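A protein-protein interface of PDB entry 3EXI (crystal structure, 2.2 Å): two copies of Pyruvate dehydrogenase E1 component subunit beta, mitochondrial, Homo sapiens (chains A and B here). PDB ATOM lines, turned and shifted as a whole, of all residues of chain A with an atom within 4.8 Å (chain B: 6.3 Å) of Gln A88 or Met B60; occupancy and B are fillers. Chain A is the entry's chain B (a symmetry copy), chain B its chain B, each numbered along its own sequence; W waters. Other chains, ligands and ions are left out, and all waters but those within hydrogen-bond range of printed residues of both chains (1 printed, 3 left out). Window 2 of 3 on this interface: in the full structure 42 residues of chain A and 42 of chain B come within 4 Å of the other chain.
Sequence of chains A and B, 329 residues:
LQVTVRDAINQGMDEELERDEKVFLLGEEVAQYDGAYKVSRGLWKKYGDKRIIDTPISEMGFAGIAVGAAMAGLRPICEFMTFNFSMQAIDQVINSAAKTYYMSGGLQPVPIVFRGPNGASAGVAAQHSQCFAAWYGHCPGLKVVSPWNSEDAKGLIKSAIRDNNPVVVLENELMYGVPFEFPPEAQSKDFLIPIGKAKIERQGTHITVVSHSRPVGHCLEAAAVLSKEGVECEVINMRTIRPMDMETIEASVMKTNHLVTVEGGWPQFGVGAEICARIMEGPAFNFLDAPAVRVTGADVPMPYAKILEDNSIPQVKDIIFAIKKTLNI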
ATOM      1  N   GLU A  59     -20.055   9.540   8.812  1.00  0.00           N
ATOM      2  CA  GLU A  59     -19.446   8.661   7.835  1.00  0.00           C
ATOM      3  C   GLU A  59     -17.995   8.323   8.169  1.00  0.00           C
ATOM      4  O   GLU A  59     -17.627   7.169   8.124  1.00  0.00           O
ATOM      5  CB  GLU A  59     -19.581   9.179   6.409  1.00  0.00           C
ATOM      6  CG  GLU A  59     -20.860   8.752   5.754  1.00  0.00           C
ATOM      7  CD  GLU A  59     -21.956   9.673   6.130  1.00  0.00           C
ATOM      8  OE1 GLU A  59     -21.621  10.767   6.703  1.00  0.00           O
ATOM      9  OE2 GLU A  59     -23.142   9.331   5.821  1.00  0.00           O
ATOM     10  N   MET A  60     -17.167   9.330   8.482  1.00  0.00           N
ATOM     11  CA  MET A  60     -15.769   9.022   8.656  1.00  0.00           C
ATOM     12  C   MET A  60     -15.677   7.989   9.810  1.00  0.00           C
ATOM     13  O   MET A  60     -15.000   6.963   9.683  1.00  0.00           O
ATOM     14  CB  MET A  60     -14.900  10.241   8.914  1.00  0.00           C
ATOM     15  CG  MET A  60     -13.449   9.778   9.212  1.00  0.00           C
ATOM     16  SD  MET A  60     -12.336   9.634   7.742  1.00  0.00           S
ATOM     17  CE  MET A  60     -11.768  11.300   7.728  1.00  0.00           C
ATOM     18  N   PHE A  85     -21.465  10.201  -0.328  1.00  0.00           N
ATOM     19  CA  PHE A  85     -21.252  10.409   1.112  1.00  0.00           C
ATOM     20  C   PHE A  85     -19.930   9.756   1.536  1.00  0.00           C
ATOM     21  O   PHE A  85     -19.409  10.080   2.611  1.00  0.00           O
ATOM     22  CB  PHE A  85     -22.403   9.821   1.964  1.00  0.00           C
ATOM     23  CG  PHE A  85     -23.800  10.402   1.644  1.00  0.00           C
ATOM     24  CD1 PHE A  85     -23.947  11.655   1.059  1.00  0.00           C
ATOM     25  CD2 PHE A  85     -24.950   9.689   1.938  1.00  0.00           C
ATOM     26  CE1 PHE A  85     -25.208  12.193   0.760  1.00  0.00           C
ATOM     27  CE2 PHE A  85     -26.245  10.230   1.650  1.00  0.00           C
ATOM     28  CZ  PHE A  85     -26.355  11.466   1.048  1.00  0.00           C
ATOM     29  N   SER A  86     -19.390   8.839   0.708  1.00  0.00           N
ATOM     30  CA  SER A  86     -18.114   8.155   0.987  1.00  0.00           C
ATOM     31  C   SER A  86     -16.983   9.147   0.980  1.00  0.00           C
ATOM     32  O   SER A  86     -15.931   8.911   1.606  1.00  0.00           O
ATOM     33  CB  SER A  86     -17.825   7.068  -0.039  1.00  0.00           C
ATOM     34  OG  SER A  86     -17.442   7.599  -1.332  1.00  0.00           O
ATOM     35  N   MET A  87     -17.167  10.272   0.298  1.00  0.00           N
ATOM     36  CA  MET A  87     -16.118  11.305   0.304  1.00  0.00           C
ATOM     37  C   MET A  87     -15.722  11.768   1.721  1.00  0.00           C
ATOM     38  O   MET A  87     -14.536  12.119   1.948  1.00  0.00           O
ATOM     39  CB  MET A  87     -16.491  12.540  -0.570  1.00  0.00           C
ATOM     40  CG  MET A  87     -16.373  12.280  -2.095  1.00  0.00           C
ATOM     41  SD  MET A  87     -16.303  13.768  -3.066  1.00  0.00           S
ATOM     42  CE  MET A  87     -17.932  14.366  -2.635  1.00  0.00           C
ATOM     43  N   GLN A  88     -16.702  11.866   2.642  1.00  0.00           N
ATOM     44  CA  GLN A  88     -16.423  12.201   4.064  1.00  0.00           C
ATOM     45  C   GLN A  88     -15.519  11.162   4.755  1.00  0.00           C
ATOM     46  O   GLN A  88     -14.789  11.468   5.672  1.00  0.00           O
ATOM     47  CB  GLN A  88     -17.714  12.337   4.877  1.00  0.00           C
ATOM     48  CG  GLN A  88     -18.653  13.445   4.381  1.00  0.00           C
ATOM     49  CD  GLN A  88     -19.486  14.030   5.476  1.00  0.00           C
ATOM     50  OE1 GLN A  88     -19.708  15.239   5.503  1.00  0.00           O
ATOM     51  NE2 GLN A  88     -19.942  13.197   6.415  1.00  0.00           N
ATOM     52  N   ALA A  89     -15.608   9.931   4.316  1.00  0.00           N
ATOM     53  CA  ALA A  89     -14.841   8.814   4.883  1.00  0.00           C
ATOM     54  C   ALA A  89     -13.659   8.336   3.989  1.00  0.00           C
ATOM     55  O   ALA A  89     -13.078   7.278   4.223  1.00  0.00           O
ATOM     56  CB  ALA A  89     -15.777   7.662   5.102  1.00  0.00           C
ATOM     57  N   ILE A  90     -13.324   9.088   2.951  1.00  0.00           N
ATOM     58  CA  ILE A  90     -12.468   8.510   1.921  1.00  0.00           C
ATOM     59  C   ILE A  90     -11.020   8.164   2.411  1.00  0.00           C
ATOM     60  O   ILE A  90     -10.432   7.143   1.976  1.00  0.00           O
ATOM     61  CB  ILE A  90     -12.502   9.319   0.572  1.00  0.00           C
ATOM     62  CG1 ILE A  90     -12.100   8.395  -0.564  1.00  0.00           C
ATOM     63  CG2 ILE A  90     -11.621  10.623   0.593  1.00  0.00           C
ATOM     64  CD1 ILE A  90     -12.789   8.716  -1.899  1.00  0.00           C
ATOM     65  N   SER B  58      -7.536  20.051  11.783  1.00  0.00           N
ATOM     66  CA  SER B  58      -8.959  19.858  11.621  1.00  0.00           C
ATOM     67  C   SER B  58      -9.259  20.089  10.163  1.00  0.00           C
ATOM     68  O   SER B  58      -9.870  21.083   9.815  1.00  0.00           O
ATOM     69  CB  SER B  58      -9.729  20.887  12.446  1.00  0.00           C
ATOM     70  OG  SER B  58      -9.531  20.666  13.819  1.00  0.00           O
ATOM     71  N   GLU B  59      -8.859  19.166   9.304  1.00  0.00           N
ATOM     72  CA  GLU B  59      -8.875  19.477   7.890  1.00  0.00           C
ATOM     73  C   GLU B  59     -10.279  19.769   7.366  1.00  0.00           C
ATOM     74  O   GLU B  59     -10.465  20.750   6.677  1.00  0.00           O
ATOM     75  CB  GLU B  59      -8.177  18.420   7.044  1.00  0.00           C
ATOM     76  CG  GLU B  59      -6.703  18.661   6.914  1.00  0.00           C
ATOM     77  CD  GLU B  59      -5.991  18.107   8.088  1.00  0.00           C
ATOM     78  OE1 GLU B  59      -6.659  17.331   8.856  1.00  0.00           O
ATOM     79  OE2 GLU B  59      -4.763  18.408   8.225  1.00  0.00           O
ATOM     80  N   MET B  60     -11.261  18.910   7.674  1.00  0.00           N
ATOM     81  CA  MET B  60     -12.549  19.114   7.060  1.00  0.00           C
ATOM     82  C   MET B  60     -13.035  20.523   7.491  1.00  0.00           C
ATOM     83  O   MET B  60     -13.473  21.320   6.655  1.00  0.00           O
ATOM     84  CB  MET B  60     -13.566  18.035   7.395  1.00  0.00           C
ATOM     85  CG  MET B  60     -14.940  18.425   6.789  1.00  0.00           C
ATOM     86  SD  MET B  60     -15.264  17.813   5.075  1.00  0.00           S
ATOM     87  CE  MET B  60     -15.938  16.249   5.519  1.00  0.00           C
ATOM     88  N   GLY B  61     -12.876  20.803   8.788  1.00  0.00           N
ATOM     89  CA  GLY B  61     -13.328  22.016   9.381  1.00  0.00           C
ATOM     90  C   GLY B  61     -12.647  23.221   8.794  1.00  0.00           C
ATOM     91  O   GLY B  61     -13.307  24.169   8.415  1.00  0.00           O
ATOM     92  N   PHE B  62     -11.335  23.237   8.690  1.00  0.00           N
ATOM     93  CA  PHE B  62     -10.759  24.519   8.278  1.00  0.00           C
ATOM     94  C   PHE B  62     -10.870  24.719   6.772  1.00  0.00           C
ATOM     95  O   PHE B  62     -10.839  25.872   6.283  1.00  0.00           O
ATOM     96  CB  PHE B  62      -9.367  24.764   8.846  1.00  0.00           C
ATOM     97  CG  PHE B  62      -8.281  23.956   8.198  1.00  0.00           C
ATOM     98  CD1 PHE B  62      -7.874  24.232   6.885  1.00  0.00           C
ATOM     99  CD2 PHE B  62      -7.580  22.980   8.943  1.00  0.00           C
ATOM    100  CE1 PHE B  62      -6.849  23.484   6.287  1.00  0.00           C
ATOM    101  CE2 PHE B  62      -6.562  22.222   8.382  1.00  0.00           C
ATOM    102  CZ  PHE B  62      -6.185  22.482   7.036  1.00  0.00           C
ATOM    103  N   ALA B  63     -11.055  23.616   6.031  1.00  0.00           N
ATOM    104  CA  ALA B  63     -11.274  23.779   4.597  1.00  0.00           C
ATOM    105  C   ALA B  63     -12.710  24.313   4.327  1.00  0.00           C
ATOM    106  O   ALA B  63     -12.893  25.129   3.446  1.00  0.00           O
ATOM    107  CB  ALA B  63     -11.035  22.456   3.840  1.00  0.00           C
ATOM    108  N   GLY B  64     -13.699  23.826   5.096  1.00  0.00           N
ATOM    109  CA  GLY B  64     -15.081  24.296   5.058  1.00  0.00           C
ATOM    110  C   GLY B  64     -15.067  25.782   5.474  1.00  0.00           C
ATOM    111  O   GLY B  64     -15.684  26.630   4.842  1.00  0.00           O
ATOM    112  N   ILE B  65     -14.382  26.097   6.569  1.00  0.00           N
ATOM    113  CA  ILE B  65     -14.253  27.499   6.966  1.00  0.00           C
ATOM    114  C   ILE B  65     -13.722  28.326   5.805  1.00  0.00           C
ATOM    115  O   ILE B  65     -14.259  29.377   5.515  1.00  0.00           O
ATOM    116  CB  ILE B  65     -13.459  27.625   8.259  1.00  0.00           C
ATOM    117  CG1 ILE B  65     -14.317  27.115   9.416  1.00  0.00           C
ATOM    118  CG2 ILE B  65     -12.936  29.028   8.507  1.00  0.00           C
ATOM    119  CD1 ILE B  65     -13.716  27.313  10.794  1.00  0.00           C
ATOM    120  N   PHE B  80      -3.127  22.851   2.347  1.00  0.00           N
ATOM    121  CA  PHE B  80      -3.128  21.494   2.904  1.00  0.00           C
ATOM    122  C   PHE B  80      -1.630  21.208   3.167  1.00  0.00           C
ATOM    123  O   PHE B  80      -0.771  21.539   2.345  1.00  0.00           O
ATOM    124  CB  PHE B  80      -3.797  20.450   1.965  1.00  0.00           C
ATOM    125  CG  PHE B  80      -5.323  20.561   1.886  1.00  0.00           C
ATOM    126  CD1 PHE B  80      -6.115  20.361   3.021  1.00  0.00           C
ATOM    127  CD2 PHE B  80      -5.962  20.911   0.694  1.00  0.00           C
ATOM    128  CE1 PHE B  80      -7.541  20.483   2.978  1.00  0.00           C
ATOM    129  CE2 PHE B  80      -7.387  20.993   0.619  1.00  0.00           C
ATOM    130  CZ  PHE B  80      -8.179  20.794   1.753  1.00  0.00           C
ATOM    131  N   MET B  87      -7.729  14.588   1.614  1.00  0.00           N
ATOM    132  CA  MET B  87      -8.774  13.551   1.593  1.00  0.00           C
ATOM    133  C   MET B  87      -9.803  13.694   2.732  1.00  0.00           C
ATOM    134  O   MET B  87     -10.996  13.350   2.533  1.00  0.00           O
ATOM    135  CB  MET B  87      -8.184  12.108   1.593  1.00  0.00           C
ATOM    136  CG  MET B  87      -7.585  11.682   0.227  1.00  0.00           C
ATOM    137  SD  MET B  87      -7.374   9.924   0.061  1.00  0.00           S
ATOM    138  CE  MET B  87      -6.177   9.742   1.378  1.00  0.00           C
ATOM    139  N   GLN B  88      -9.350  14.100   3.935  1.00  0.00           N
ATOM    140  CA  GLN B  88     -10.265  14.374   5.076  1.00  0.00           C
ATOM    141  C   GLN B  88     -11.266  15.507   4.779  1.00  0.00           C
ATOM    142  O   GLN B  88     -12.355  15.544   5.308  1.00  0.00           O
ATOM    143  CB  GLN B  88      -9.491  14.733   6.348  1.00  0.00           C
ATOM    144  CG  GLN B  88      -8.552  13.625   6.844  1.00  0.00           C
ATOM    145  CD  GLN B  88      -8.358  13.651   8.325  1.00  0.00           C
ATOM    146  OE1 GLN B  88      -8.300  12.598   8.959  1.00  0.00           O
ATOM    147  NE2 GLN B  88      -8.281  14.847   8.915  1.00  0.00           N
ATOM    148  N   ALA B  89     -10.863  16.436   3.950  1.00  0.00           N
ATOM    149  CA  ALA B  89     -11.680  17.601   3.582  1.00  0.00           C
ATOM    150  C   ALA B  89     -12.285  17.526   2.149  1.00  0.00           C
ATOM    151  O   ALA B  89     -12.794  18.516   1.626  1.00  0.00           O
ATOM    152  CB  ALA B  89     -10.822  18.828   3.681  1.00  0.00           C
ATOM    153  N   ILE B  90     -12.201  16.374   1.500  1.00  0.00           N
ATOM    154  CA  ILE B  90     -12.446  16.366   0.063  1.00  0.00           C
ATOM    155  C   ILE B  90     -13.914  16.734  -0.340  1.00  0.00           C
ATOM    156  O   ILE B  90     -14.137  17.405  -1.378  1.00  0.00           O
ATOM    157  CB  ILE B  90     -11.901  15.070  -0.644  1.00  0.00           C
ATOM    158  CG1 ILE B  90     -11.657  15.376  -2.111  1.00  0.00           C
ATOM    159  CG2 ILE B  90     -12.832  13.813  -0.465  1.00  0.00           C
ATOM    160  CD1 ILE B  90     -10.486  14.593  -2.723  1.00  0.00           C
ATOM    161  N   ASP B  91     -14.887  16.378   0.501  1.00  0.00           N
ATOM    162  CA  ASP B  91     -16.249  16.784   0.240  1.00  0.00           C
ATOM    163  C   ASP B  91     -16.437  18.337   0.209  1.00  0.00           C
ATOM    164  O   ASP B  91     -17.138  18.893  -0.602  1.00  0.00           O
ATOM    165  CB  ASP B  91     -17.138  16.161   1.280  1.00  0.00           C
ATOM    166  CG  ASP B  91     -18.604  16.567   1.107  1.00  0.00           C
ATOM    167  OD1 ASP B  91     -19.328  15.854   0.345  1.00  0.00           O
ATOM    168  OD2 ASP B  91     -19.036  17.540   1.798  1.00  0.00           O
ATOM    169  N   GLN B  92     -15.737  19.042   1.069  1.00  0.00           N
ATOM    170  CA  GLN B  92     -15.721  20.500   1.000  1.00  0.00           C
ATOM    171  C   GLN B  92     -15.184  20.995  -0.339  1.00  0.00           C
ATOM    172  O   GLN B  92     -15.759  21.914  -0.935  1.00  0.00           O
ATOM    173  CB  GLN B  92     -14.921  21.117   2.186  1.00  0.00           C
ATOM    174  CG  GLN B  92     -15.662  20.930   3.556  1.00  0.00           C
ATOM    175  CD  GLN B  92     -16.992  21.733   3.681  1.00  0.00           C
ATOM    176  OE1 GLN B  92     -17.394  22.419   2.752  1.00  0.00           O
ATOM    177  NE2 GLN B  92     -17.641  21.675   4.853  1.00  0.00           N
HETATM  178  O   HOH W   1      -9.034  10.049   8.635  1.00  0.00           O
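The side-chain carboxylate (OE1) of Glu B59 lies within hydrogen-bond range of the side-chain amide nitrogen (NE2) of Gln B88 (3.0 Å).
The side-chain carboxylate of Glu A59 sits at hydrogen-bond distance from the side-chain amide nitrogen of Gln A88 (3.0 Å).
Of the printed residues of chain A, Met B60 touches Gln A88.
Of the printed residues of chain A, Met B87 touches Met A87 (3.8 Å) and Ile A90 (3.4 Å).
Of the printed residues of chain A, Gln B88 touches Met A60 (3.9 Å).
Of the printed residues of chain B, Met A87 touches Met B87 (3.8 Å), Ile B90 (3.4 Å) and Asp B91 (3.6 Å).
Printed residues of chain A within 4 Å of Ile B90: Met A87 and Ile A90.
Ala B63 touches none of the printed residues of chain A.
Ser B58 touches none of the printed residues of chain A.
The nearest printed residue of chain A that does not touch Met B60 is Met A87 (5.6 Å).
The nearest printed residue of chain B that does not touch Met A60 is Met B87 (5.6 Å).
Hydrophobic or aromatic side chains of chain B that line the printed part of chain A: Met B60, Met B87 and Ile B90.
Of the 8 printed residues of chain A, 4 touch a printed residue of chain B.
Hydrophobic or aromatic side chains of chain A that line the printed part of chain B: Met A60, Met A87 and Ile A90.
Among the printed residues, no Asp or Glu carboxylate lies within 4 Å of a Lys or Arg side-chain nitrogen of the other chain.
Water W1 bridges OE1 of Gln B88 (2.7 Å) and SD of Met A60 (3.4 Å).
Met A60 touches Gln B88, and with the chains exchanged Gln A88 touches Met B60.
Met A87 touches its own counterpart, Met B87.
Met A87 touches Ile B90, and with the chains exchanged Ile A90 touches Met B87.
Ile A90 touches its own counterpart, Ile B90.
6 positions are printed for both chains.
Of the 7 pairs that touch across the chains among the printed residues, 6 have their exchanged pair printed and touching as well.
Gln B88 touches Met A60 (OE1 to CE, 3.9 Å).
Met B87 touches Met A87.
Met A87 touches Ile B90.
Met A87 touches Asp B91 (CE to OD1, 3.6 Å).
CE of Met B60 touches OE1 of Gln A88, at 3.9 Å.
Ile A90 touches Met B87.
Ile A90 touches Ile B90.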
